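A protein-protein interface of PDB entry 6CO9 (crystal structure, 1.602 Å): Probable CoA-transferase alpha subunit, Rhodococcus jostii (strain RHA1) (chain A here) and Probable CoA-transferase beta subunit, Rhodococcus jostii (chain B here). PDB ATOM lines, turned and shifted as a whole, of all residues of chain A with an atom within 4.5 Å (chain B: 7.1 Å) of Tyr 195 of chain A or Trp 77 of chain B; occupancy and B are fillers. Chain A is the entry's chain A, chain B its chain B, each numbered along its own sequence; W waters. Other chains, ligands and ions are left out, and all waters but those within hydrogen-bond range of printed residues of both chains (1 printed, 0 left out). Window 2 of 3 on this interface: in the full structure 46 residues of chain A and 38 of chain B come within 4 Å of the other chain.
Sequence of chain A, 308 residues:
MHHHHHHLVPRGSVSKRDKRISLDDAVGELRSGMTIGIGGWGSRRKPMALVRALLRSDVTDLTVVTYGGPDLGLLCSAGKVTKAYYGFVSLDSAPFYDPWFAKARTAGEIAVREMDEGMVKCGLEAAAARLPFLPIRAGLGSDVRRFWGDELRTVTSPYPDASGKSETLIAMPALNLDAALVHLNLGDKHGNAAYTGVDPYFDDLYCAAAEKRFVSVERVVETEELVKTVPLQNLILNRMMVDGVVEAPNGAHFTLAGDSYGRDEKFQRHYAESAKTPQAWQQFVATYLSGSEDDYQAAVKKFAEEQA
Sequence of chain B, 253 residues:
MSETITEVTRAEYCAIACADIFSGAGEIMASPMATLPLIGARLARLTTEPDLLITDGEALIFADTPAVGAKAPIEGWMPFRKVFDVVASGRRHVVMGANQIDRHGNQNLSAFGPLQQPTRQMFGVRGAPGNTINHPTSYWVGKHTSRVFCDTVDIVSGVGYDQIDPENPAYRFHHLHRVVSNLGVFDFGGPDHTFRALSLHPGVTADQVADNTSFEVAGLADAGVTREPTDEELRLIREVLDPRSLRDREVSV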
ATOM      1  N   ARG A  45     -21.869  13.854 -33.000  1.00  0.00           N
ATOM      2  CA  ARG A  45     -20.543  13.440 -32.532  1.00  0.00           C
ATOM      3  C   ARG A  45     -20.065  12.161 -33.205  1.00  0.00           C
ATOM      4  O   ARG A  45     -19.589  11.223 -32.571  1.00  0.00           O
ATOM      5  CB  ARG A  45     -20.498  13.304 -31.002  1.00  0.00           C
ATOM      6  CG  ARG A  45     -19.107  13.676 -30.465  1.00  0.00           C
ATOM      7  CD  ARG A  45     -18.992  13.595 -28.940  1.00  0.00           C
ATOM      8  NE  ARG A  45     -19.182  12.218 -28.499  1.00  0.00           N
ATOM      9  CZ  ARG A  45     -20.103  11.809 -27.629  1.00  0.00           C
ATOM     10  NH1 ARG A  45     -20.927  12.678 -27.040  1.00  0.00           N
ATOM     11  NH2 ARG A  45     -20.183  10.510 -27.344  1.00  0.00           N
ATOM     12  N   LEU A 184     -14.650  11.961 -28.951  1.00  0.00           N
ATOM     13  CA  LEU A 184     -15.028  12.564 -27.679  1.00  0.00           C
ATOM     14  C   LEU A 184     -14.396  13.947 -27.559  1.00  0.00           C
ATOM     15  O   LEU A 184     -13.591  14.372 -28.397  1.00  0.00           O
ATOM     16  CB  LEU A 184     -14.632  11.651 -26.508  1.00  0.00           C
ATOM     17  CG  LEU A 184     -15.562  10.444 -26.341  1.00  0.00           C
ATOM     18  CD1 LEU A 184     -14.958   9.412 -25.404  1.00  0.00           C
ATOM     19  CD2 LEU A 184     -16.949  10.895 -25.831  1.00  0.00           C
ATOM     20  N   ASN A 185     -14.793  14.677 -26.522  1.00  0.00           N
ATOM     21  CA  ASN A 185     -14.416  16.080 -26.427  1.00  0.00           C
ATOM     22  C   ASN A 185     -13.034  16.299 -25.825  1.00  0.00           C
ATOM     23  O   ASN A 185     -12.366  17.272 -26.178  1.00  0.00           O
ATOM     24  CB  ASN A 185     -15.473  16.836 -25.617  1.00  0.00           C
ATOM     25  CG  ASN A 185     -16.838  16.758 -26.258  1.00  0.00           C
ATOM     26  OD1 ASN A 185     -17.622  15.860 -25.952  1.00  0.00           O
ATOM     27  ND2 ASN A 185     -17.102  17.661 -27.206  1.00  0.00           N
ATOM     28  N   ALA A 194     -13.471  11.901 -22.002  1.00  0.00           N
ATOM     29  CA  ALA A 194     -14.732  12.408 -21.488  1.00  0.00           C
ATOM     30  C   ALA A 194     -15.548  13.034 -22.608  1.00  0.00           C
ATOM     31  O   ALA A 194     -14.999  13.548 -23.590  1.00  0.00           O
ATOM     32  CB  ALA A 194     -14.510  13.447 -20.378  1.00  0.00           C
ATOM     33  N   TYR A 195     -16.868  13.000 -22.440  1.00  0.00           N
ATOM     34  CA  TYR A 195     -17.774  13.830 -23.215  1.00  0.00           C
ATOM     35  C   TYR A 195     -18.151  15.072 -22.418  1.00  0.00           C
ATOM     36  O   TYR A 195     -18.182  15.068 -21.183  1.00  0.00           O
ATOM     37  CB  TYR A 195     -19.041  13.071 -23.622  1.00  0.00           C
ATOM     38  CG  TYR A 195     -20.041  12.844 -22.518  1.00  0.00           C
ATOM     39  CD1 TYR A 195     -19.851  11.829 -21.610  1.00  0.00           C
ATOM     40  CD2 TYR A 195     -21.183  13.639 -22.406  1.00  0.00           C
ATOM     41  CE1 TYR A 195     -20.764  11.606 -20.601  1.00  0.00           C
ATOM     42  CE2 TYR A 195     -22.109  13.425 -21.403  1.00  0.00           C
ATOM     43  CZ  TYR A 195     -21.894  12.402 -20.503  1.00  0.00           C
ATOM     44  OH  TYR A 195     -22.801  12.152 -19.484  1.00  0.00           O
ATOM     45  N   THR A 196     -18.422  16.144 -23.146  1.00  0.00           N
ATOM     46  CA  THR A 196     -18.976  17.372 -22.605  1.00  0.00           C
ATOM     47  C   THR A 196     -20.246  17.670 -23.379  1.00  0.00           C
ATOM     48  O   THR A 196     -20.263  17.584 -24.611  1.00  0.00           O
ATOM     49  CB  THR A 196     -18.001  18.545 -22.732  1.00  0.00           C
ATOM     50  OG1 THR A 196     -17.669  18.721 -24.115  1.00  0.00           O
ATOM     51  CG2 THR A 196     -16.735  18.273 -21.945  1.00  0.00           C
ATOM     52  N   GLY A 197     -21.298  18.027 -22.677  1.00  0.00           N
ATOM     53  CA  GLY A 197     -22.590  18.147 -23.315  1.00  0.00           C
ATOM     54  C   GLY A 197     -23.595  17.231 -22.654  1.00  0.00           C
ATOM     55  O   GLY A 197     -23.351  16.659 -21.586  1.00  0.00           O
ATOM     56  N   VAL A 198     -24.753  17.098 -23.297  1.00  0.00           N
ATOM     57  CA  VAL A 198     -25.890  16.478 -22.621  1.00  0.00           C
ATOM     58  C   VAL A 198     -26.002  14.974 -22.839  1.00  0.00           C
ATOM     59  O   VAL A 198     -26.841  14.334 -22.189  1.00  0.00           O
ATOM     60  CB  VAL A 198     -27.221  17.133 -23.041  1.00  0.00           C
ATOM     61  CG1 VAL A 198     -27.226  18.631 -22.701  1.00  0.00           C
ATOM     62  CG2 VAL A 198     -27.504  16.904 -24.514  1.00  0.00           C
ATOM     63  N   ASP A 199     -25.189  14.376 -23.713  1.00  0.00           N
ATOM     64  CA  ASP A 199     -25.423  12.959 -23.970  1.00  0.00           C
ATOM     65  C   ASP A 199     -24.127  12.223 -24.307  1.00  0.00           C
ATOM     66  O   ASP A 199     -23.426  12.613 -25.247  1.00  0.00           O
ATOM     67  CB  ASP A 199     -26.447  12.822 -25.108  1.00  0.00           C
ATOM     68  CG  ASP A 199     -27.121  11.459 -25.149  1.00  0.00           C
ATOM     69  OD1 ASP A 199     -26.478  10.448 -24.790  1.00  0.00           O
ATOM     70  OD2 ASP A 199     -28.310  11.389 -25.552  1.00  0.00           O
ATOM     71  N   PRO A 200     -23.785  11.144 -23.589  1.00  0.00           N
ATOM     72  CA  PRO A 200     -22.630  10.322 -23.994  1.00  0.00           C
ATOM     73  C   PRO A 200     -22.884   9.464 -25.233  1.00  0.00           C
ATOM     74  O   PRO A 200     -21.935   8.850 -25.757  1.00  0.00           O
ATOM     75  CB  PRO A 200     -22.402   9.429 -22.767  1.00  0.00           C
ATOM     76  CG  PRO A 200     -23.798   9.209 -22.247  1.00  0.00           C
ATOM     77  CD  PRO A 200     -24.468  10.583 -22.404  1.00  0.00           C
ATOM     78  N   GLN A 233     -18.697  11.662 -13.651  1.00  0.00           N
ATOM     79  CA  GLN A 233     -19.628  10.868 -14.434  1.00  0.00           C
ATOM     80  C   GLN A 233     -19.388  11.016 -15.926  1.00  0.00           C
ATOM     81  O   GLN A 233     -19.858  10.185 -16.708  1.00  0.00           O
ATOM     82  CB  GLN A 233     -21.065  11.255 -14.064  1.00  0.00           C
ATOM     83  CG  GLN A 233     -21.472  10.880 -12.634  1.00  0.00           C
ATOM     84  CD  GLN A 233     -20.951  11.833 -11.548  1.00  0.00           C
ATOM     85  OE1 GLN A 233     -20.319  12.850 -11.828  1.00  0.00           O
ATOM     86  NE2 GLN A 233     -21.215  11.488 -10.293  1.00  0.00           N
ATOM     87  N   ASN A 234     -18.643  12.039 -16.331  1.00  0.00           N
ATOM     88  CA  ASN A 234     -18.350  12.259 -17.736  1.00  0.00           C
ATOM     89  C   ASN A 234     -17.140  11.476 -18.216  1.00  0.00           C
ATOM     90  O   ASN A 234     -16.875  11.457 -19.420  1.00  0.00           O
ATOM     91  CB  ASN A 234     -18.120  13.751 -17.993  1.00  0.00           C
ATOM     92  CG  ASN A 234     -19.378  14.580 -17.805  1.00  0.00           C
ATOM     93  OD1 ASN A 234     -19.904  14.691 -16.703  1.00  0.00           O
ATOM     94  ND2 ASN A 234     -19.882  15.146 -18.887  1.00  0.00           N
ATOM     95  N   ILE A 236     -16.081   8.624 -19.381  1.00  0.00           N
ATOM     96  CA  ILE A 236     -16.725   7.389 -19.829  1.00  0.00           C
ATOM     97  C   ILE A 236     -15.756   6.360 -20.406  1.00  0.00           C
ATOM     98  O   ILE A 236     -16.117   5.176 -20.481  1.00  0.00           O
ATOM     99  CB  ILE A 236     -17.870   7.634 -20.837  1.00  0.00           C
ATOM    100  CG1 ILE A 236     -17.388   8.278 -22.136  1.00  0.00           C
ATOM    101  CG2 ILE A 236     -18.999   8.460 -20.188  1.00  0.00           C
ATOM    102  CD1 ILE A 236     -18.483   8.277 -23.206  1.00  0.00           C
ATOM    103  N   THR B  55     -39.860  15.922 -22.693  1.00  0.00           N
ATOM    104  CA  THR B  55     -38.463  16.278 -22.897  1.00  0.00           C
ATOM    105  C   THR B  55     -38.339  17.375 -23.942  1.00  0.00           C
ATOM    106  O   THR B  55     -39.309  17.748 -24.611  1.00  0.00           O
ATOM    107  CB  THR B  55     -37.633  15.072 -23.343  1.00  0.00           C
ATOM    108  OG1 THR B  55     -37.967  14.740 -24.697  1.00  0.00           O
ATOM    109  CG2 THR B  55     -37.903  13.876 -22.448  1.00  0.00           C
ATOM    110  N   ALA B  59     -32.249  15.510 -24.651  1.00  0.00           N
ATOM    111  CA  ALA B  59     -31.786  14.783 -23.472  1.00  0.00           C
ATOM    112  C   ALA B  59     -32.239  15.395 -22.148  1.00  0.00           C
ATOM    113  O   ALA B  59     -31.802  14.944 -21.085  1.00  0.00           O
ATOM    114  CB  ALA B  59     -30.257  14.687 -23.475  1.00  0.00           C
ATOM    115  N   LEU B  60     -33.087  16.419 -22.174  1.00  0.00           N
ATOM    116  CA  LEU B  60     -33.483  17.099 -20.947  1.00  0.00           C
ATOM    117  C   LEU B  60     -34.975  16.916 -20.710  1.00  0.00           C
ATOM    118  O   LEU B  60     -35.780  17.054 -21.631  1.00  0.00           O
ATOM    119  CB  LEU B  60     -33.138  18.599 -20.989  1.00  0.00           C
ATOM    120  CG  LEU B  60     -31.666  18.960 -21.216  1.00  0.00           C
ATOM    121  CD1 LEU B  60     -31.495  20.457 -21.380  1.00  0.00           C
ATOM    122  CD2 LEU B  60     -30.765  18.424 -20.125  1.00  0.00           C
ATOM    123  N   ILE B  61     -35.336  16.580 -19.472  1.00  0.00           N
ATOM    124  CA  ILE B  61     -36.726  16.505 -19.042  1.00  0.00           C
ATOM    125  C   ILE B  61     -37.148  17.880 -18.548  1.00  0.00           C
ATOM    126  O   ILE B  61     -36.499  18.449 -17.665  1.00  0.00           O
ATOM    127  CB  ILE B  61     -36.891  15.455 -17.930  1.00  0.00           C
ATOM    128  CG1 ILE B  61     -36.152  14.151 -18.250  1.00  0.00           C
ATOM    129  CG2 ILE B  61     -38.387  15.250 -17.582  1.00  0.00           C
ATOM    130  CD1 ILE B  61     -36.418  13.055 -17.169  1.00  0.00           C
ATOM    131  N   ILE B  74     -35.573  22.697 -16.269  1.00  0.00           N
ATOM    132  CA  ILE B  74     -35.548  21.243 -16.389  1.00  0.00           C
ATOM    133  C   ILE B  74     -35.792  20.597 -15.032  1.00  0.00           C
ATOM    134  O   ILE B  74     -35.676  21.226 -13.975  1.00  0.00           O
ATOM    135  CB  ILE B  74     -34.221  20.744 -16.988  1.00  0.00           C
ATOM    136  CG1 ILE B  74     -33.078  20.975 -16.002  1.00  0.00           C
ATOM    137  CG2 ILE B  74     -33.948  21.429 -18.328  1.00  0.00           C
ATOM    138  CD1 ILE B  74     -31.879  20.078 -16.250  1.00  0.00           C
ATOM    139  N   GLU B  75     -36.133  19.303 -15.075  1.00  0.00           N
ATOM    140  CA  GLU B  75     -36.316  18.527 -13.858  1.00  0.00           C
ATOM    141  C   GLU B  75     -35.557  17.208 -13.860  1.00  0.00           C
ATOM    142  O   GLU B  75     -35.621  16.485 -12.859  1.00  0.00           O
ATOM    143  CB  GLU B  75     -37.808  18.233 -13.595  1.00  0.00           C
ATOM    144  CG  GLU B  75     -38.422  17.247 -14.593  1.00  0.00           C
ATOM    145  CD  GLU B  75     -39.819  16.794 -14.205  1.00  0.00           C
ATOM    146  OE1 GLU B  75     -40.316  17.221 -13.135  1.00  0.00           O
ATOM    147  OE2 GLU B  75     -40.410  15.993 -14.967  1.00  0.00           O
ATOM    148  N   GLY B  76     -34.853  16.870 -14.934  1.00  0.00           N
ATOM    149  CA  GLY B  76     -34.148  15.599 -14.954  1.00  0.00           C
ATOM    150  C   GLY B  76     -33.418  15.400 -16.260  1.00  0.00           C
ATOM    151  O   GLY B  76     -33.433  16.259 -17.150  1.00  0.00           O
ATOM    152  N   TRP B  77     -32.726  14.269 -16.337  1.00  0.00           N
ATOM    153  CA  TRP B  77     -31.869  13.893 -17.459  1.00  0.00           C
ATOM    154  C   TRP B  77     -32.382  12.674 -18.196  1.00  0.00           C
ATOM    155  O   TRP B  77     -32.709  11.702 -17.602  1.00  0.00           O
ATOM    156  CB  TRP B  77     -30.462  13.666 -16.939  1.00  0.00           C
ATOM    157  CG  TRP B  77     -29.374  13.520 -17.959  1.00  0.00           C
ATOM    158  CD1 TRP B  77     -29.199  14.273 -19.082  1.00  0.00           C
ATOM    159  CD2 TRP B  77     -28.309  12.578 -17.940  1.00  0.00           C
ATOM    160  NE1 TRP B  77     -28.097  13.855 -19.757  1.00  0.00           N
ATOM    161  CE2 TRP B  77     -27.531  12.812 -19.090  1.00  0.00           C
ATOM    162  CE3 TRP B  77     -27.939  11.547 -17.092  1.00  0.00           C
ATOM    163  CZ2 TRP B  77     -26.425  12.058 -19.386  1.00  0.00           C
ATOM    164  CZ3 TRP B  77     -26.860  10.808 -17.401  1.00  0.00           C
ATOM    165  CH2 TRP B  77     -26.102  11.060 -18.556  1.00  0.00           C
ATOM    166  N   MET B  78     -32.427  12.762 -19.518  1.00  0.00           N
ATOM    167  CA  MET B  78     -32.945  11.684 -20.311  1.00  0.00           C
ATOM    168  C   MET B  78     -32.160  11.501 -21.608  1.00  0.00           C
ATOM    169  O   MET B  78     -32.682  11.653 -22.663  1.00  0.00           O
ATOM    170  CB  MET B  78     -34.409  11.900 -20.595  1.00  0.00           C
ATOM    171  CG  MET B  78     -35.151  10.818 -21.303  1.00  0.00           C
ATOM    172  SD  MET B  78     -35.157   9.198 -20.502  1.00  0.00           S
ATOM    173  CE  MET B  78     -35.860   9.583 -18.886  1.00  0.00           C
ATOM    174  N   PRO B  79     -30.932  11.071 -21.475  1.00  0.00           N
ATOM    175  CA  PRO B  79     -30.110  10.757 -22.640  1.00  0.00           C
ATOM    176  C   PRO B  79     -30.652   9.529 -23.399  1.00  0.00           C
ATOM    177  O   PRO B  79     -31.374   8.738 -22.914  1.00  0.00           O
ATOM    178  CB  PRO B  79     -28.759  10.471 -22.041  1.00  0.00           C
ATOM    179  CG  PRO B  79     -29.081   9.948 -20.666  1.00  0.00           C
ATOM    180  CD  PRO B  79     -30.202  10.806 -20.237  1.00  0.00           C
ATOM    181  N   PHE B  80     -30.194   9.351 -24.619  1.00  0.00           N
ATOM    182  CA  PHE B  80     -30.794   8.308 -25.444  1.00  0.00           C
ATOM    183  C   PHE B  80     -30.681   6.924 -24.797  1.00  0.00           C
ATOM    184  O   PHE B  80     -31.619   6.121 -24.878  1.00  0.00           O
ATOM    185  CB  PHE B  80     -30.170   8.318 -26.840  1.00  0.00           C
ATOM    186  CG  PHE B  80     -30.581   9.494 -27.683  1.00  0.00           C
ATOM    187  CD1 PHE B  80     -31.729  10.212 -27.400  1.00  0.00           C
ATOM    188  CD2 PHE B  80     -29.830   9.853 -28.782  1.00  0.00           C
ATOM    189  CE1 PHE B  80     -32.102  11.295 -28.197  1.00  0.00           C
ATOM    190  CE2 PHE B  80     -30.193  10.918 -29.586  1.00  0.00           C
ATOM    191  CZ  PHE B  80     -31.326  11.637 -29.310  1.00  0.00           C
ATOM    192  N   ARG B  81     -29.559   6.620 -24.133  1.00  0.00           N
ATOM    193  CA  ARG B  81     -29.445   5.283 -23.540  1.00  0.00           C
ATOM    194  C   ARG B  81     -30.504   5.063 -22.464  1.00  0.00           C
ATOM    195  O   ARG B  81     -31.003   3.942 -22.286  1.00  0.00           O
ATOM    196  CB  ARG B  81     -28.042   5.056 -22.971  1.00  0.00           C
ATOM    197  CG  ARG B  81     -27.647   5.977 -21.814  1.00  0.00           C
ATOM    198  CD  ARG B  81     -26.131   6.121 -21.785  1.00  0.00           C
ATOM    199  NE  ARG B  81     -25.485   4.872 -21.388  1.00  0.00           N
ATOM    200  CZ  ARG B  81     -24.282   4.472 -21.800  1.00  0.00           C
ATOM    201  NH1 ARG B  81     -23.581   5.202 -22.669  1.00  0.00           N
ATOM    202  NH2 ARG B  81     -23.783   3.320 -21.359  1.00  0.00           N
ATOM    203  N   LYS B  82     -30.874   6.118 -21.755  1.00  0.00           N
ATOM    204  CA  LYS B  82     -31.879   5.977 -20.722  1.00  0.00           C
ATOM    205  C   LYS B  82     -33.293   5.935 -21.333  1.00  0.00           C
ATOM    206  O   LYS B  82     -34.203   5.359 -20.731  1.00  0.00           O
ATOM    207  CB  LYS B  82     -31.635   7.106 -19.703  1.00  0.00           C
ATOM    208  CG  LYS B  82     -32.147   6.997 -18.285  1.00  0.00           C
ATOM    209  CD  LYS B  82     -31.976   8.393 -17.642  1.00  0.00           C
ATOM    210  CE  LYS B  82     -31.054   8.402 -16.460  1.00  0.00           C
ATOM    211  NZ  LYS B  82     -29.677   8.101 -16.919  1.00  0.00           N
HETATM  212  O   HOH W   1     -27.069   7.892 -24.450  1.00  0.00           O
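The backbone carbonyl oxygen (O) of Val 198 of chain A sits at hydrogen-bond distance from the indole nitrogen (NE1) of Trp 77 of chain B. OD2 of Asp 199 of chain A is in hydrogen-bond range of N of Phe 80 of chain B (2.9 Å).
The backbone NH of Met 78 of chain B is in hydrogen-bond range of the backbone carbonyl oxygen of Ala 59 of chain B, at 2.8 Å. ND2 of Asn 234 of chain A sits at hydrogen-bond distance from O of Tyr 195 of chain A, 2.9 Å away. The guanidinium group of Arg 45 of chain A is in hydrogen-bond range of the backbone carbonyl oxygen of Pro 200 of chain A, 2.9 Å away. The backbone carbonyl oxygen of Asp 199 of chain A lies within hydrogen-bond range of the guanidinium group of Arg 45 of chain A.
Among the printed residues, merely in contact across the chains: Tyr 195 of chain A with Trp 77 of chain B (3.6 Å), Val 198 of chain A with Ala 59 of chain B (3.7 Å), Asp 199 of chain A with Pro 79 of chain B (3.5 Å), Pro 200 of chain A with Trp 77 of chain B (3.9 Å) and Pro 200 of chain A with Arg 81 of chain B (3.9 Å).
Tyr 195 of chain A touches just one residue of chain B: Trp 77 (3.6 Å). Trp 77 of chain B touches just these residues of chain A: Tyr 195 (3.6 Å), Val 198 (2.8 Å) and Pro 200 (3.9 Å). Of the printed residues of chain A, Arg 81 of chain B touches Pro 200 (3.9 Å). Of the printed residues of chain B, Asp 199 of chain A touches Pro 79 (3.5 Å) and Phe 80 (2.9 Å). Of the printed residues of chain B, Pro 200 of chain A touches Trp 77 and Arg 81. The nearest residue of chain B that does not touch Tyr 195 of chain A is Pro 79 of chain B (6.7 Å). The nearest printed residue of chain A that does not touch Trp 77 of chain B is Asp 199 of chain A (4.8 Å). The nearest printed residue of chain A that does not touch Phe 80 of chain B is Pro 200 of chain A (6.3 Å).
Printed residues of chain A that touch a printed residue of chain B: Tyr 195, Val 198, Asp 199 and Pro 200. Hydrophobic or aromatic side chains of chain A within 4 Å of the printed part of chain B: Tyr 195, Val 198 and Pro 200. Printed residues of chain B that touch a printed residue of chain A: Ala 59, Trp 77, Pro 79, Phe 80 and Arg 81. Hydrophobic or aromatic side chains of chain B that line the printed part of chain A: Ala 59, Trp 77, Pro 79 and Phe 80. Along chain B the printed residues that touch a printed residue of chain A span positions 59 to 81. Among the printed residues, 7 pairs touch across the chains. Among the printed residues, no Asp or Glu carboxylate lies within 4 Å of a Lys or Arg side-chain nitrogen of the other chain.
Water W1 lies within hydrogen-bond range of OD1 of Asp 199 of chain A (2.6 Å), N of Arg 81 of chain B (2.8 Å) and N of Phe 80 of chain B (3.5 Å).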
